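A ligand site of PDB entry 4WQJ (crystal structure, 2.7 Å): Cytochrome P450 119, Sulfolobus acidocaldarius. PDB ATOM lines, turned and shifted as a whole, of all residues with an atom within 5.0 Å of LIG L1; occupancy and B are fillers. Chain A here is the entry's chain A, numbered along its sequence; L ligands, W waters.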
ATOM      1  N   LEU A  33      29.766 -10.538  33.359  1.00  0.00           N
ATOM      2  CA  LEU A  33      28.433 -10.449  32.760  1.00  0.00           C
ATOM      3  C   LEU A  33      27.508  -9.461  33.482  1.00  0.00           C
ATOM      4  O   LEU A  33      26.754  -8.743  32.841  1.00  0.00           O
ATOM      5  CB  LEU A  33      27.762 -11.820  32.719  1.00  0.00           C
ATOM      6  CG  LEU A  33      28.447 -12.768  31.721  1.00  0.00           C
ATOM      7  CD1 LEU A  33      27.763 -14.123  31.625  1.00  0.00           C
ATOM      8  CD2 LEU A  33      28.530 -12.112  30.381  1.00  0.00           C
ATOM      9  N   MET A  68      19.884  -4.355  20.639  1.00  0.00           N
ATOM     10  CA  MET A  68      20.007  -4.460  22.083  1.00  0.00           C
ATOM     11  C   MET A  68      21.182  -5.339  22.537  1.00  0.00           C
ATOM     12  O   MET A  68      21.681  -5.199  23.647  1.00  0.00           O
ATOM     13  CB  MET A  68      18.701  -4.989  22.665  1.00  0.00           C
ATOM     14  CG  MET A  68      18.497  -6.490  22.494  1.00  0.00           C
ATOM     15  SD  MET A  68      16.946  -7.012  23.265  1.00  0.00           S
ATOM     16  CE  MET A  68      15.721  -6.530  22.044  1.00  0.00           C
ATOM     17  N   LEU A  69      21.629  -6.248  21.677  1.00  0.00           N
ATOM     18  CA  LEU A  69      22.689  -7.170  22.085  1.00  0.00           C
ATOM     19  C   LEU A  69      23.986  -6.423  22.304  1.00  0.00           C
ATOM     20  O   LEU A  69      24.799  -6.805  23.145  1.00  0.00           O
ATOM     21  CB  LEU A  69      22.865  -8.273  21.043  1.00  0.00           C
ATOM     22  CG  LEU A  69      23.929  -9.339  21.309  1.00  0.00           C
ATOM     23  CD1 LEU A  69      23.602 -10.234  22.525  1.00  0.00           C
ATOM     24  CD2 LEU A  69      24.089 -10.158  20.063  1.00  0.00           C
ATOM     25  N   HIS A  76      19.901  -0.042  26.101  1.00  0.00           N
ATOM     26  CA  HIS A  76      19.569  -1.435  26.100  1.00  0.00           C
ATOM     27  C   HIS A  76      18.196  -1.678  26.713  1.00  0.00           C
ATOM     28  O   HIS A  76      17.367  -2.403  26.150  1.00  0.00           O
ATOM     29  CB  HIS A  76      20.616  -2.248  26.867  1.00  0.00           C
ATOM     30  CG  HIS A  76      20.132  -3.619  27.236  1.00  0.00           C
ATOM     31  ND1 HIS A  76      19.480  -3.873  28.424  1.00  0.00           N
ATOM     32  CD2 HIS A  76      20.145  -4.777  26.554  1.00  0.00           C
ATOM     33  CE1 HIS A  76      19.149  -5.152  28.467  1.00  0.00           C
ATOM     34  NE2 HIS A  76      19.552  -5.722  27.343  1.00  0.00           N
ATOM     35  N   ARG A  80      14.943  -3.243  24.848  1.00  0.00           N
ATOM     36  CA  ARG A  80      14.431  -4.516  25.311  1.00  0.00           C
ATOM     37  C   ARG A  80      13.001  -4.428  25.820  1.00  0.00           C
ATOM     38  O   ARG A  80      12.195  -5.359  25.669  1.00  0.00           O
ATOM     39  CB  ARG A  80      15.335  -5.051  26.416  1.00  0.00           C
ATOM     40  CG  ARG A  80      14.803  -6.319  27.057  1.00  0.00           C
ATOM     41  CD  ARG A  80      15.936  -7.179  27.584  1.00  0.00           C
ATOM     42  NE  ARG A  80      15.407  -8.410  28.154  1.00  0.00           N
ATOM     43  CZ  ARG A  80      16.114  -9.516  28.399  1.00  0.00           C
ATOM     44  NH1 ARG A  80      17.416  -9.564  28.128  1.00  0.00           N
ATOM     45  NH2 ARG A  80      15.495 -10.557  28.913  1.00  0.00           N
ATOM     46  N   PHE A  87       8.064 -12.307  25.141  1.00  0.00           N
ATOM     47  CA  PHE A  87       8.907 -13.489  25.395  1.00  0.00           C
ATOM     48  C   PHE A  87       8.911 -13.969  26.846  1.00  0.00           C
ATOM     49  O   PHE A  87       9.727 -14.806  27.226  1.00  0.00           O
ATOM     50  CB  PHE A  87      10.342 -13.227  24.914  1.00  0.00           C
ATOM     51  CG  PHE A  87      10.416 -13.029  23.439  1.00  0.00           C
ATOM     52  CD1 PHE A  87      10.441 -14.130  22.584  1.00  0.00           C
ATOM     53  CD2 PHE A  87      10.380 -11.751  22.898  1.00  0.00           C
ATOM     54  CE1 PHE A  87      10.473 -13.950  21.204  1.00  0.00           C
ATOM     55  CE2 PHE A  87      10.400 -11.563  21.517  1.00  0.00           C
ATOM     56  CZ  PHE A  87      10.447 -12.668  20.671  1.00  0.00           C
ATOM     57  N   ILE A 130       9.150 -19.117  15.560  1.00  0.00           N
ATOM     58  CA  ILE A 130       9.501 -17.707  15.618  1.00  0.00           C
ATOM     59  C   ILE A 130       8.743 -16.980  14.507  1.00  0.00           C
ATOM     60  O   ILE A 130       8.335 -15.813  14.662  1.00  0.00           O
ATOM     61  CB  ILE A 130      11.035 -17.460  15.500  1.00  0.00           C
ATOM     62  CG1 ILE A 130      11.397 -16.041  15.969  1.00  0.00           C
ATOM     63  CG2 ILE A 130      11.533 -17.689  14.100  1.00  0.00           C
ATOM     64  CD1 ILE A 130      11.210 -15.813  17.438  1.00  0.00           C
ATOM     65  N   LEU A 205      17.353  -9.518  14.276  1.00  0.00           N
ATOM     66  CA  LEU A 205      17.836 -10.116  15.499  1.00  0.00           C
ATOM     67  C   LEU A 205      16.821 -11.126  16.063  1.00  0.00           C
ATOM     68  O   LEU A 205      17.173 -12.281  16.288  1.00  0.00           O
ATOM     69  CB  LEU A 205      18.123  -9.046  16.523  1.00  0.00           C
ATOM     70  CG  LEU A 205      18.692  -9.691  17.787  1.00  0.00           C
ATOM     71  CD1 LEU A 205      20.019 -10.330  17.461  1.00  0.00           C
ATOM     72  CD2 LEU A 205      18.820  -8.717  18.931  1.00  0.00           C
ATOM     73  N   LEU A 206      15.576 -10.708  16.265  1.00  0.00           N
ATOM     74  CA  LEU A 206      14.532 -11.616  16.747  1.00  0.00           C
ATOM     75  C   LEU A 206      14.226 -12.772  15.777  1.00  0.00           C
ATOM     76  O   LEU A 206      14.066 -13.917  16.189  1.00  0.00           O
ATOM     77  CB  LEU A 206      13.242 -10.854  17.036  1.00  0.00           C
ATOM     78  CG  LEU A 206      13.232  -9.807  18.152  1.00  0.00           C
ATOM     79  CD1 LEU A 206      11.814  -9.325  18.363  1.00  0.00           C
ATOM     80  CD2 LEU A 206      13.800 -10.356  19.433  1.00  0.00           C
ATOM     81  N   GLY A 210      18.102 -16.512  17.130  1.00  0.00           N
ATOM     82  CA  GLY A 210      17.832 -17.607  18.055  1.00  0.00           C
ATOM     83  C   GLY A 210      17.574 -18.984  17.456  1.00  0.00           C
ATOM     84  O   GLY A 210      17.366 -19.963  18.187  1.00  0.00           O
ATOM     85  N   THR A 213      20.844 -21.629  17.585  1.00  0.00           N
ATOM     86  CA  THR A 213      21.143 -21.927  18.999  1.00  0.00           C
ATOM     87  C   THR A 213      20.121 -22.897  19.607  1.00  0.00           C
ATOM     88  O   THR A 213      20.468 -23.751  20.445  1.00  0.00           O
ATOM     89  CB  THR A 213      21.176 -20.635  19.871  1.00  0.00           C
ATOM     90  OG1 THR A 213      20.049 -19.817  19.571  1.00  0.00           O
ATOM     91  CG2 THR A 213      22.448 -19.835  19.654  1.00  0.00           C
ATOM     92  N   THR A 214      18.871 -22.779  19.208  1.00  0.00           N
ATOM     93  CA  THR A 214      17.842 -23.641  19.748  1.00  0.00           C
ATOM     94  C   THR A 214      17.908 -25.026  19.125  1.00  0.00           C
ATOM     95  O   THR A 214      17.867 -26.053  19.833  1.00  0.00           O
ATOM     96  CB  THR A 214      16.456 -23.012  19.513  1.00  0.00           C
ATOM     97  OG1 THR A 214      16.461 -21.699  20.081  1.00  0.00           O
ATOM     98  CG2 THR A 214      15.350 -23.841  20.170  1.00  0.00           C
ATOM     99  N   LEU A 217      20.343 -26.842  20.970  1.00  0.00           N
ATOM    100  CA  LEU A 217      19.931 -27.301  22.298  1.00  0.00           C
ATOM    101  C   LEU A 217      19.174 -28.602  22.179  1.00  0.00           C
ATOM    102  O   LEU A 217      19.340 -29.517  22.986  1.00  0.00           O
ATOM    103  CB  LEU A 217      19.078 -26.261  23.007  1.00  0.00           C
ATOM    104  CG  LEU A 217      18.375 -26.766  24.275  1.00  0.00           C
ATOM    105  CD1 LEU A 217      19.346 -27.271  25.321  1.00  0.00           C
ATOM    106  CD2 LEU A 217      17.519 -25.662  24.854  1.00  0.00           C
ATOM    107  N   LEU A 248      21.742 -28.062  28.966  1.00  0.00           N
ATOM    108  CA  LEU A 248      22.157 -26.668  28.852  1.00  0.00           C
ATOM    109  C   LEU A 248      23.480 -26.400  29.571  1.00  0.00           C
ATOM    110  O   LEU A 248      24.362 -25.747  29.010  1.00  0.00           O
ATOM    111  CB  LEU A 248      21.089 -25.729  29.377  1.00  0.00           C
ATOM    112  CG  LEU A 248      20.021 -25.385  28.344  1.00  0.00           C
ATOM    113  CD1 LEU A 248      18.777 -24.857  29.039  1.00  0.00           C
ATOM    114  CD2 LEU A 248      20.557 -24.384  27.342  1.00  0.00           C
ATOM    115  N   PRO A 253      24.898 -24.473  23.924  1.00  0.00           N
ATOM    116  CA  PRO A 253      24.891 -24.083  22.496  1.00  0.00           C
ATOM    117  C   PRO A 253      25.735 -22.837  22.200  1.00  0.00           C
ATOM    118  O   PRO A 253      26.248 -22.726  21.098  1.00  0.00           O
ATOM    119  CB  PRO A 253      23.413 -23.806  22.205  1.00  0.00           C
ATOM    120  CG  PRO A 253      22.679 -24.535  23.242  1.00  0.00           C
ATOM    121  CD  PRO A 253      23.541 -24.477  24.475  1.00  0.00           C
ATOM    122  N   VAL A 254      25.829 -21.896  23.128  1.00  0.00           N
ATOM    123  CA  VAL A 254      26.786 -20.789  23.006  1.00  0.00           C
ATOM    124  C   VAL A 254      27.904 -20.991  24.028  1.00  0.00           C
ATOM    125  O   VAL A 254      27.626 -21.134  25.217  1.00  0.00           O
ATOM    126  CB  VAL A 254      26.091 -19.427  23.206  1.00  0.00           C
ATOM    127  CG1 VAL A 254      27.098 -18.286  23.099  1.00  0.00           C
ATOM    128  CG2 VAL A 254      24.971 -19.264  22.194  1.00  0.00           C
ATOM    129  N   THR A 257      31.138 -15.615  25.262  1.00  0.00           N
ATOM    130  CA  THR A 257      30.689 -14.327  24.779  1.00  0.00           C
ATOM    131  C   THR A 257      31.784 -13.334  25.154  1.00  0.00           C
ATOM    132  O   THR A 257      32.789 -13.738  25.732  1.00  0.00           O
ATOM    133  CB  THR A 257      29.324 -13.950  25.363  1.00  0.00           C
ATOM    134  OG1 THR A 257      28.832 -12.779  24.717  1.00  0.00           O
ATOM    135  CG2 THR A 257      29.423 -13.697  26.846  1.00  0.00           C
ATOM    136  N   VAL A 258      31.603 -12.052  24.841  1.00  0.00           N
ATOM    137  CA  VAL A 258      32.680 -11.083  24.985  1.00  0.00           C
ATOM    138  C   VAL A 258      32.205  -9.726  25.540  1.00  0.00           C
ATOM    139  O   VAL A 258      31.060  -9.331  25.317  1.00  0.00           O
ATOM    140  CB  VAL A 258      33.388 -10.892  23.607  1.00  0.00           C
ATOM    141  CG1 VAL A 258      32.358 -10.557  22.550  1.00  0.00           C
ATOM    142  CG2 VAL A 258      34.451  -9.800  23.661  1.00  0.00           C
ATOM    143  N   ARG A 259      33.063  -9.036  26.295  1.00  0.00           N
ATOM    144  CA  ARG A 259      32.808  -7.655  26.728  1.00  0.00           C
ATOM    145  C   ARG A 259      34.028  -6.784  26.449  1.00  0.00           C
ATOM    146  O   ARG A 259      35.096  -7.296  26.161  1.00  0.00           O
ATOM    147  CB  ARG A 259      32.453  -7.589  28.220  1.00  0.00           C
ATOM    148  CG  ARG A 259      31.176  -8.327  28.630  1.00  0.00           C
ATOM    149  CD  ARG A 259      29.931  -7.636  28.088  1.00  0.00           C
ATOM    150  NE  ARG A 259      28.708  -8.245  28.615  1.00  0.00           N
ATOM    151  CZ  ARG A 259      28.064  -9.237  28.008  1.00  0.00           C
ATOM    152  NH1 ARG A 259      28.537  -9.733  26.876  1.00  0.00           N
ATOM    153  NH2 ARG A 259      26.963  -9.749  28.544  1.00  0.00           N
ATOM    154  N   ILE A 282      31.627 -19.227  28.990  1.00  0.00           N
ATOM    155  CA  ILE A 282      30.436 -19.811  29.600  1.00  0.00           C
ATOM    156  C   ILE A 282      30.563 -21.319  29.830  1.00  0.00           C
ATOM    157  O   ILE A 282      30.114 -21.831  30.855  1.00  0.00           O
ATOM    158  CB  ILE A 282      29.211 -19.547  28.713  1.00  0.00           C
ATOM    159  CG1 ILE A 282      28.922 -18.051  28.707  1.00  0.00           C
ATOM    160  CG2 ILE A 282      27.977 -20.357  29.187  1.00  0.00           C
ATOM    161  CD1 ILE A 282      27.853 -17.692  27.743  1.00  0.00           C
ATOM    162  N   LEU A 308      25.203 -20.681  33.333  1.00  0.00           N
ATOM    163  CA  LEU A 308      25.232 -19.401  32.647  1.00  0.00           C
ATOM    164  C   LEU A 308      24.988 -19.529  31.143  1.00  0.00           C
ATOM    165  O   LEU A 308      25.271 -18.604  30.384  1.00  0.00           O
ATOM    166  CB  LEU A 308      26.576 -18.723  32.898  1.00  0.00           C
ATOM    167  CG  LEU A 308      26.938 -18.600  34.375  1.00  0.00           C
ATOM    168  CD1 LEU A 308      28.386 -18.155  34.564  1.00  0.00           C
ATOM    169  CD2 LEU A 308      25.973 -17.667  35.116  1.00  0.00           C
ATOM    170  N   SER A 309      24.414 -20.648  30.703  1.00  0.00           N
ATOM    171  CA  SER A 309      24.201 -20.887  29.285  1.00  0.00           C
ATOM    172  C   SER A 309      23.289 -19.844  28.597  1.00  0.00           C
ATOM    173  O   SER A 309      23.343 -19.677  27.382  1.00  0.00           O
ATOM    174  CB  SER A 309      23.616 -22.279  29.080  1.00  0.00           C
ATOM    175  OG  SER A 309      24.534 -23.265  29.504  1.00  0.00           O
ATOM    176  N   PHE A 310      22.460 -19.170  29.372  1.00  0.00           N
ATOM    177  CA  PHE A 310      21.675 -18.079  28.799  1.00  0.00           C
ATOM    178  C   PHE A 310      22.256 -16.734  29.172  1.00  0.00           C
ATOM    179  O   PHE A 310      21.659 -15.693  28.917  1.00  0.00           O
ATOM    180  CB  PHE A 310      20.220 -18.162  29.260  1.00  0.00           C
ATOM    181  CG  PHE A 310      19.441 -19.261  28.616  1.00  0.00           C
ATOM    182  CD1 PHE A 310      19.225 -19.259  27.252  1.00  0.00           C
ATOM    183  CD2 PHE A 310      18.912 -20.311  29.390  1.00  0.00           C
ATOM    184  CE1 PHE A 310      18.495 -20.285  26.656  1.00  0.00           C
ATOM    185  CE2 PHE A 310      18.178 -21.356  28.809  1.00  0.00           C
ATOM    186  CZ  PHE A 310      17.967 -21.333  27.440  1.00  0.00           C
ATOM    187  N   GLY A 311      23.444 -16.746  29.772  1.00  0.00           N
ATOM    188  CA  GLY A 311      24.044 -15.517  30.264  1.00  0.00           C
ATOM    189  C   GLY A 311      23.548 -15.163  31.664  1.00  0.00           C
ATOM    190  O   GLY A 311      23.045 -16.008  32.404  1.00  0.00           O
ATOM    191  N   ILE A 314      21.746  -8.012  32.753  1.00  0.00           N
ATOM    192  CA  ILE A 314      20.739  -7.341  31.921  1.00  0.00           C
ATOM    193  C   ILE A 314      20.612  -7.948  30.509  1.00  0.00           C
ATOM    194  O   ILE A 314      19.629  -7.687  29.827  1.00  0.00           O
ATOM    195  CB  ILE A 314      21.026  -5.834  31.766  1.00  0.00           C
ATOM    196  CG1 ILE A 314      22.353  -5.600  31.057  1.00  0.00           C
ATOM    197  CG2 ILE A 314      20.959  -5.089  33.120  1.00  0.00           C
ATOM    198  CD1 ILE A 314      22.627  -4.176  30.820  1.00  0.00           C
ATOM    199  N   HIS A 315      21.580  -8.753  30.058  1.00  0.00           N
ATOM    200  CA  HIS A 315      21.475  -9.302  28.700  1.00  0.00           C
ATOM    201  C   HIS A 315      20.993 -10.736  28.689  1.00  0.00           C
ATOM    202  O   HIS A 315      20.964 -11.361  27.631  1.00  0.00           O
ATOM    203  CB  HIS A 315      22.810  -9.228  27.968  1.00  0.00           C
ATOM    204  CG  HIS A 315      23.226  -7.828  27.643  1.00  0.00           C
ATOM    205  ND1 HIS A 315      22.725  -7.141  26.557  1.00  0.00           N
ATOM    206  CD2 HIS A 315      24.061  -6.982  28.280  1.00  0.00           C
ATOM    207  CE1 HIS A 315      23.264  -5.933  26.533  1.00  0.00           C
ATOM    208  NE2 HIS A 315      24.079  -5.806  27.559  1.00  0.00           N
ATOM    209  N   LEU A 316      20.668 -11.262  29.876  1.00  0.00           N
ATOM    210  CA  LEU A 316      20.138 -12.611  30.007  1.00  0.00           C
ATOM    211  C   LEU A 316      19.129 -12.906  28.905  1.00  0.00           C
ATOM    212  O   LEU A 316      18.221 -12.105  28.672  1.00  0.00           O
ATOM    213  CB  LEU A 316      19.479 -12.818  31.361  1.00  0.00           C
ATOM    214  CG  LEU A 316      18.876 -14.207  31.513  1.00  0.00           C
ATOM    215  CD1 LEU A 316      19.948 -15.239  31.789  1.00  0.00           C
ATOM    216  CD2 LEU A 316      17.871 -14.167  32.627  1.00  0.00           C
ATOM    217  N   CYS A 317      19.318 -14.024  28.208  1.00  0.00           N
ATOM    218  CA  CYS A 317      18.691 -14.278  26.927  1.00  0.00           C
ATOM    219  C   CYS A 317      17.181 -14.011  26.903  1.00  0.00           C
ATOM    220  O   CYS A 317      16.380 -14.718  27.528  1.00  0.00           O
ATOM    221  CB  CYS A 317      18.966 -15.729  26.487  1.00  0.00           C
ATOM    222  SG  CYS A 317      18.269 -16.145  24.860  1.00  0.00           S
ATOM    223  N   LEU A 318      16.811 -12.990  26.131  1.00  0.00           N
ATOM    224  CA  LEU A 318      15.414 -12.671  25.870  1.00  0.00           C
ATOM    225  C   LEU A 318      14.584 -13.914  25.508  1.00  0.00           C
ATOM    226  O   LEU A 318      13.424 -14.050  25.908  1.00  0.00           O
ATOM    227  CB  LEU A 318      15.318 -11.635  24.753  1.00  0.00           C
ATOM    228  CG  LEU A 318      13.910 -11.126  24.467  1.00  0.00           C
ATOM    229  CD1 LEU A 318      13.382 -10.351  25.683  1.00  0.00           C
ATOM    230  CD2 LEU A 318      13.842 -10.278  23.184  1.00  0.00           C
ATOM    231  N   GLY A 319      15.203 -14.821  24.748  1.00  0.00           N
ATOM    232  CA  GLY A 319      14.516 -16.004  24.257  1.00  0.00           C
ATOM    233  C   GLY A 319      14.619 -17.222  25.158  1.00  0.00           C
ATOM    234  O   GLY A 319      14.212 -18.311  24.760  1.00  0.00           O
ATOM    235  N   LEU A 322      11.333 -19.129  25.724  1.00  0.00           N
ATOM    236  CA  LEU A 322      10.929 -19.752  24.470  1.00  0.00           C
ATOM    237  C   LEU A 322      11.786 -21.010  24.231  1.00  0.00           C
ATOM    238  O   LEU A 322      11.246 -22.085  23.962  1.00  0.00           O
ATOM    239  CB  LEU A 322      11.047 -18.758  23.312  1.00  0.00           C
ATOM    240  CG  LEU A 322      10.664 -19.271  21.923  1.00  0.00           C
ATOM    241  CD1 LEU A 322       9.263 -19.836  21.955  1.00  0.00           C
ATOM    242  CD2 LEU A 322      10.796 -18.183  20.854  1.00  0.00           C
ATOM    243  N   ALA A 323      13.102 -20.876  24.350  1.00  0.00           N
ATOM    244  CA  ALA A 323      14.010 -21.978  24.065  1.00  0.00           C
ATOM    245  C   ALA A 323      13.777 -23.180  24.990  1.00  0.00           C
ATOM    246  O   ALA A 323      13.758 -24.324  24.538  1.00  0.00           O
ATOM    247  CB  ALA A 323      15.488 -21.510  24.150  1.00  0.00           C
HETATM  248  C1  LIG L   1      21.164 -13.151  24.592  1.00  0.00           C
HETATM  249  C2  LIG L   1      22.081 -17.925  24.592  1.00  0.00           C
HETATM  250  C3  LIG L   1      17.931 -18.796  22.238  1.00  0.00           C
HETATM  251  C4  LIG L   1      17.502 -14.040  21.515  1.00  0.00           C
HETATM  252  C5  LIG L   1      21.770 -14.364  24.815  1.00  0.00           C
HETATM  253  C6  LIG L   1      23.004 -14.586  25.554  1.00  0.00           C
HETATM  254  C7  LIG L   1      23.245 -15.907  25.545  1.00  0.00           C
HETATM  255  C8  LIG L   1      22.181 -16.567  24.813  1.00  0.00           C
HETATM  256  C9  LIG L   1      24.434 -16.636  26.198  1.00  0.00           C
HETATM  257  C10 LIG L   1      23.874 -13.505  26.232  1.00  0.00           C
HETATM  258  C11 LIG L   1      24.624 -12.617  25.247  1.00  0.00           C
HETATM  259  C12 LIG L   1      25.652 -11.799  26.018  1.00  0.00           C
HETATM  260  O1  LIG L   1      25.430 -11.507  27.237  1.00  0.00           O
HETATM  261  O2  LIG L   1      26.688 -11.431  25.402  1.00  0.00           O
HETATM  262  C13 LIG L   1      21.012 -18.573  24.013  1.00  0.00           C
HETATM  263  C14 LIG L   1      20.788 -20.011  24.007  1.00  0.00           C
HETATM  264  C15 LIG L   1      19.650 -20.237  23.323  1.00  0.00           C
HETATM  265  C16 LIG L   1      19.104 -18.960  22.919  1.00  0.00           C
HETATM  266  C17 LIG L   1      21.754 -21.052  24.655  1.00  0.00           C
HETATM  267  C18 LIG L   1      18.923 -21.565  23.009  1.00  0.00           C
HETATM  268  C19 LIG L   1      19.225 -22.724  23.586  1.00  0.00           C
HETATM  269  C20 LIG L   1      17.412 -17.578  21.875  1.00  0.00           C
HETATM  270  C21 LIG L   1      16.138 -17.310  21.234  1.00  0.00           C
HETATM  271  C22 LIG L   1      16.058 -15.979  21.062  1.00  0.00           C
HETATM  272  C23 LIG L   1      17.263 -15.385  21.561  1.00  0.00           C
HETATM  273  C24 LIG L   1      15.062 -18.361  20.861  1.00  0.00           C
HETATM  274  C25 LIG L   1      14.990 -15.067  20.429  1.00  0.00           C
HETATM  275  C26 LIG L   1      14.055 -15.479  19.585  1.00  0.00           C
HETATM  276  C27 LIG L   1      18.406 -13.359  22.287  1.00  0.00           C
HETATM  277  C28 LIG L   1      18.458 -11.928  22.361  1.00  0.00           C
HETATM  278  C29 LIG L   1      19.598 -11.638  23.331  1.00  0.00           C
HETATM  279  C30 LIG L   1      20.123 -12.933  23.721  1.00  0.00           C
HETATM  280  C31 LIG L   1      17.555 -10.898  21.654  1.00  0.00           C
HETATM  281  C32 LIG L   1      20.056 -10.256  23.785  1.00  0.00           C
HETATM  282  C33 LIG L   1      19.128  -9.814  24.913  1.00  0.00           C
HETATM  283  C34 LIG L   1      19.718  -8.567  25.538  1.00  0.00           C
HETATM  284  O3  LIG L   1      20.828  -8.138  25.093  1.00  0.00           O
HETATM  285  O4  LIG L   1      19.089  -8.007  26.478  1.00  0.00           O
HETATM  286  N1  LIG L   1      21.295 -15.599  24.379  1.00  0.00           N
HETATM  287  N2  LIG L   1      19.971 -17.968  23.338  1.00  0.00           N
HETATM  288  N3  LIG L   1      18.079 -16.377  22.042  1.00  0.00           N
HETATM  289  N4  LIG L   1      19.390 -13.917  23.083  1.00  0.00           N
HETATM  290 FE1  LIG L   1      19.691 -15.931  23.134  1.00  0.00          FE
HETATM  291  C1  LG2 L   2      20.328 -16.156  20.412  1.00  0.00           C
HETATM  292  C2  LG2 L   2      22.146 -15.818  21.594  1.00  0.00           C
HETATM  293  C3  LG2 L   2      22.520 -15.963  20.254  1.00  0.00           C
HETATM  294  C4  LG2 L   2      23.917 -15.942  19.650  1.00  0.00           C
HETATM  295  C5  LG2 L   2      25.047 -15.542  20.375  1.00  0.00           C
HETATM  296  C6  LG2 L   2      26.318 -15.564  19.780  1.00  0.00           C
HETATM  297  C7  LG2 L   2      26.470 -15.994  18.460  1.00  0.00           C
HETATM  298  C8  LG2 L   2      25.343 -16.414  17.739  1.00  0.00           C
HETATM  299 BR1  LG2 L   2      28.188 -16.047  17.588  1.00  0.00          BR
HETATM  300  C9  LG2 L   2      24.081 -16.391  18.333  1.00  0.00           C
HETATM  301  N1  LG2 L   2      21.362 -16.180  19.581  1.00  0.00           N
HETATM  302  N2  LG2 L   2      20.785 -15.936  21.633  1.00  0.00           N
HETATM  303  O   HOH W   1      24.276 -12.043  30.014  1.00  0.00           O
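SG of Cys 317 binds FE1 of LIG L1 (2.2 Å). NE2 of His 76 is in hydrogen-bond range of O4 of LIG L1 (2.5 Å). An oxygen (O3) of LIG L1 lies within hydrogen-bond range of a ring nitrogen (ND1) of His 315 (2.6 Å). OG1 of Thr 257 sits at hydrogen-bond distance from O2 of LIG L1. NH2 of Arg 259 lies within salt-bridge range of O1 of LIG L1, at 2.7 Å. The guanidinium group of Arg 80 is in salt-bridge range of an oxygen (O4) of LIG L1, 2.8 Å away.
A nitrogen (N2) of LG2 L2 is bound to an iron atom (FE1) of LIG L1 (1.9 Å).
N of Cys 317 sits at hydrogen-bond distance from O of Phe 310. The side-chain sulfur of Cys 317 sits close to the backbone NH of Gly 319, at 3.3 Å. A ring nitrogen (NE2) of His 76 lies close to the backbone carbonyl oxygen (O) of Ile 314. The guanidinium group of Arg 80 lies within hydrogen-bond range of the backbone carbonyl oxygen of Ile 314. O of Leu 316 is in hydrogen-bond range of NH1 of Arg 80 (2.7 Å). The side-chain hydroxyl (OG) of Ser 309 lies within hydrogen-bond range of the backbone carbonyl oxygen (O) of Leu 248, 2.5 Å away. The side-chain hydroxyl (OG1) of Thr 213 sits at hydrogen-bond distance from the backbone carbonyl oxygen (O) of Gly 210, 3.0 Å away. The backbone carbonyl oxygen (O) of Gly 210 is in hydrogen-bond range of the side-chain hydroxyl (OG1) of Thr 214, 2.7 Å away.
O of Met 68 sits close to O3 of LIG L1. An oxygen (O4) of LIG L1 lies close to the backbone carbonyl oxygen (O) of Ile 314 (3.4 Å). Leu 69 touches LIG L1 (CA to O3, 3.7 Å). Ile 130 touches LIG L1 (CD1 to C26, 3.6 Å). Leu 205 touches LIG L1. Leu 206 touches LIG L1. Gly 210 touches LIG L1. O of Thr 213 touches C19 of LIG L1, 3.5 Å away. Thr 214 touches LIG L1. CB of Leu 217 touches C19 of LIG L1 (3.6 Å). Pro 253 touches LIG L1. CG2 of Val 254 touches C2 of LIG L1 (3.99 Å). Ile 282 touches LIG L1. Ser 309 touches LIG L1 (O to C9, 3.4 Å). Phe 310 touches LIG L1. Gly 311 touches LIG L1 (N to C9, 3.7 Å). Leu 318 touches LIG L1 (CB to C31, 3.9 Å). Gly 319 touches LIG L1 (CA to C22, 3.5 Å). CB of Ala 323 touches C18 of LIG L1 (3.6 Å). Hydrophobic or aromatic side chains that line LIG L1: Met 68, Leu 69, His 76, Ile 130, Leu 205, Leu 217, Pro 253, Val 254, Ile 282, Phe 310, His 315, Leu 318 and Ala 323. The nearest printed residue that does not touch LIG L1 is Phe 87 (4.2 Å).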
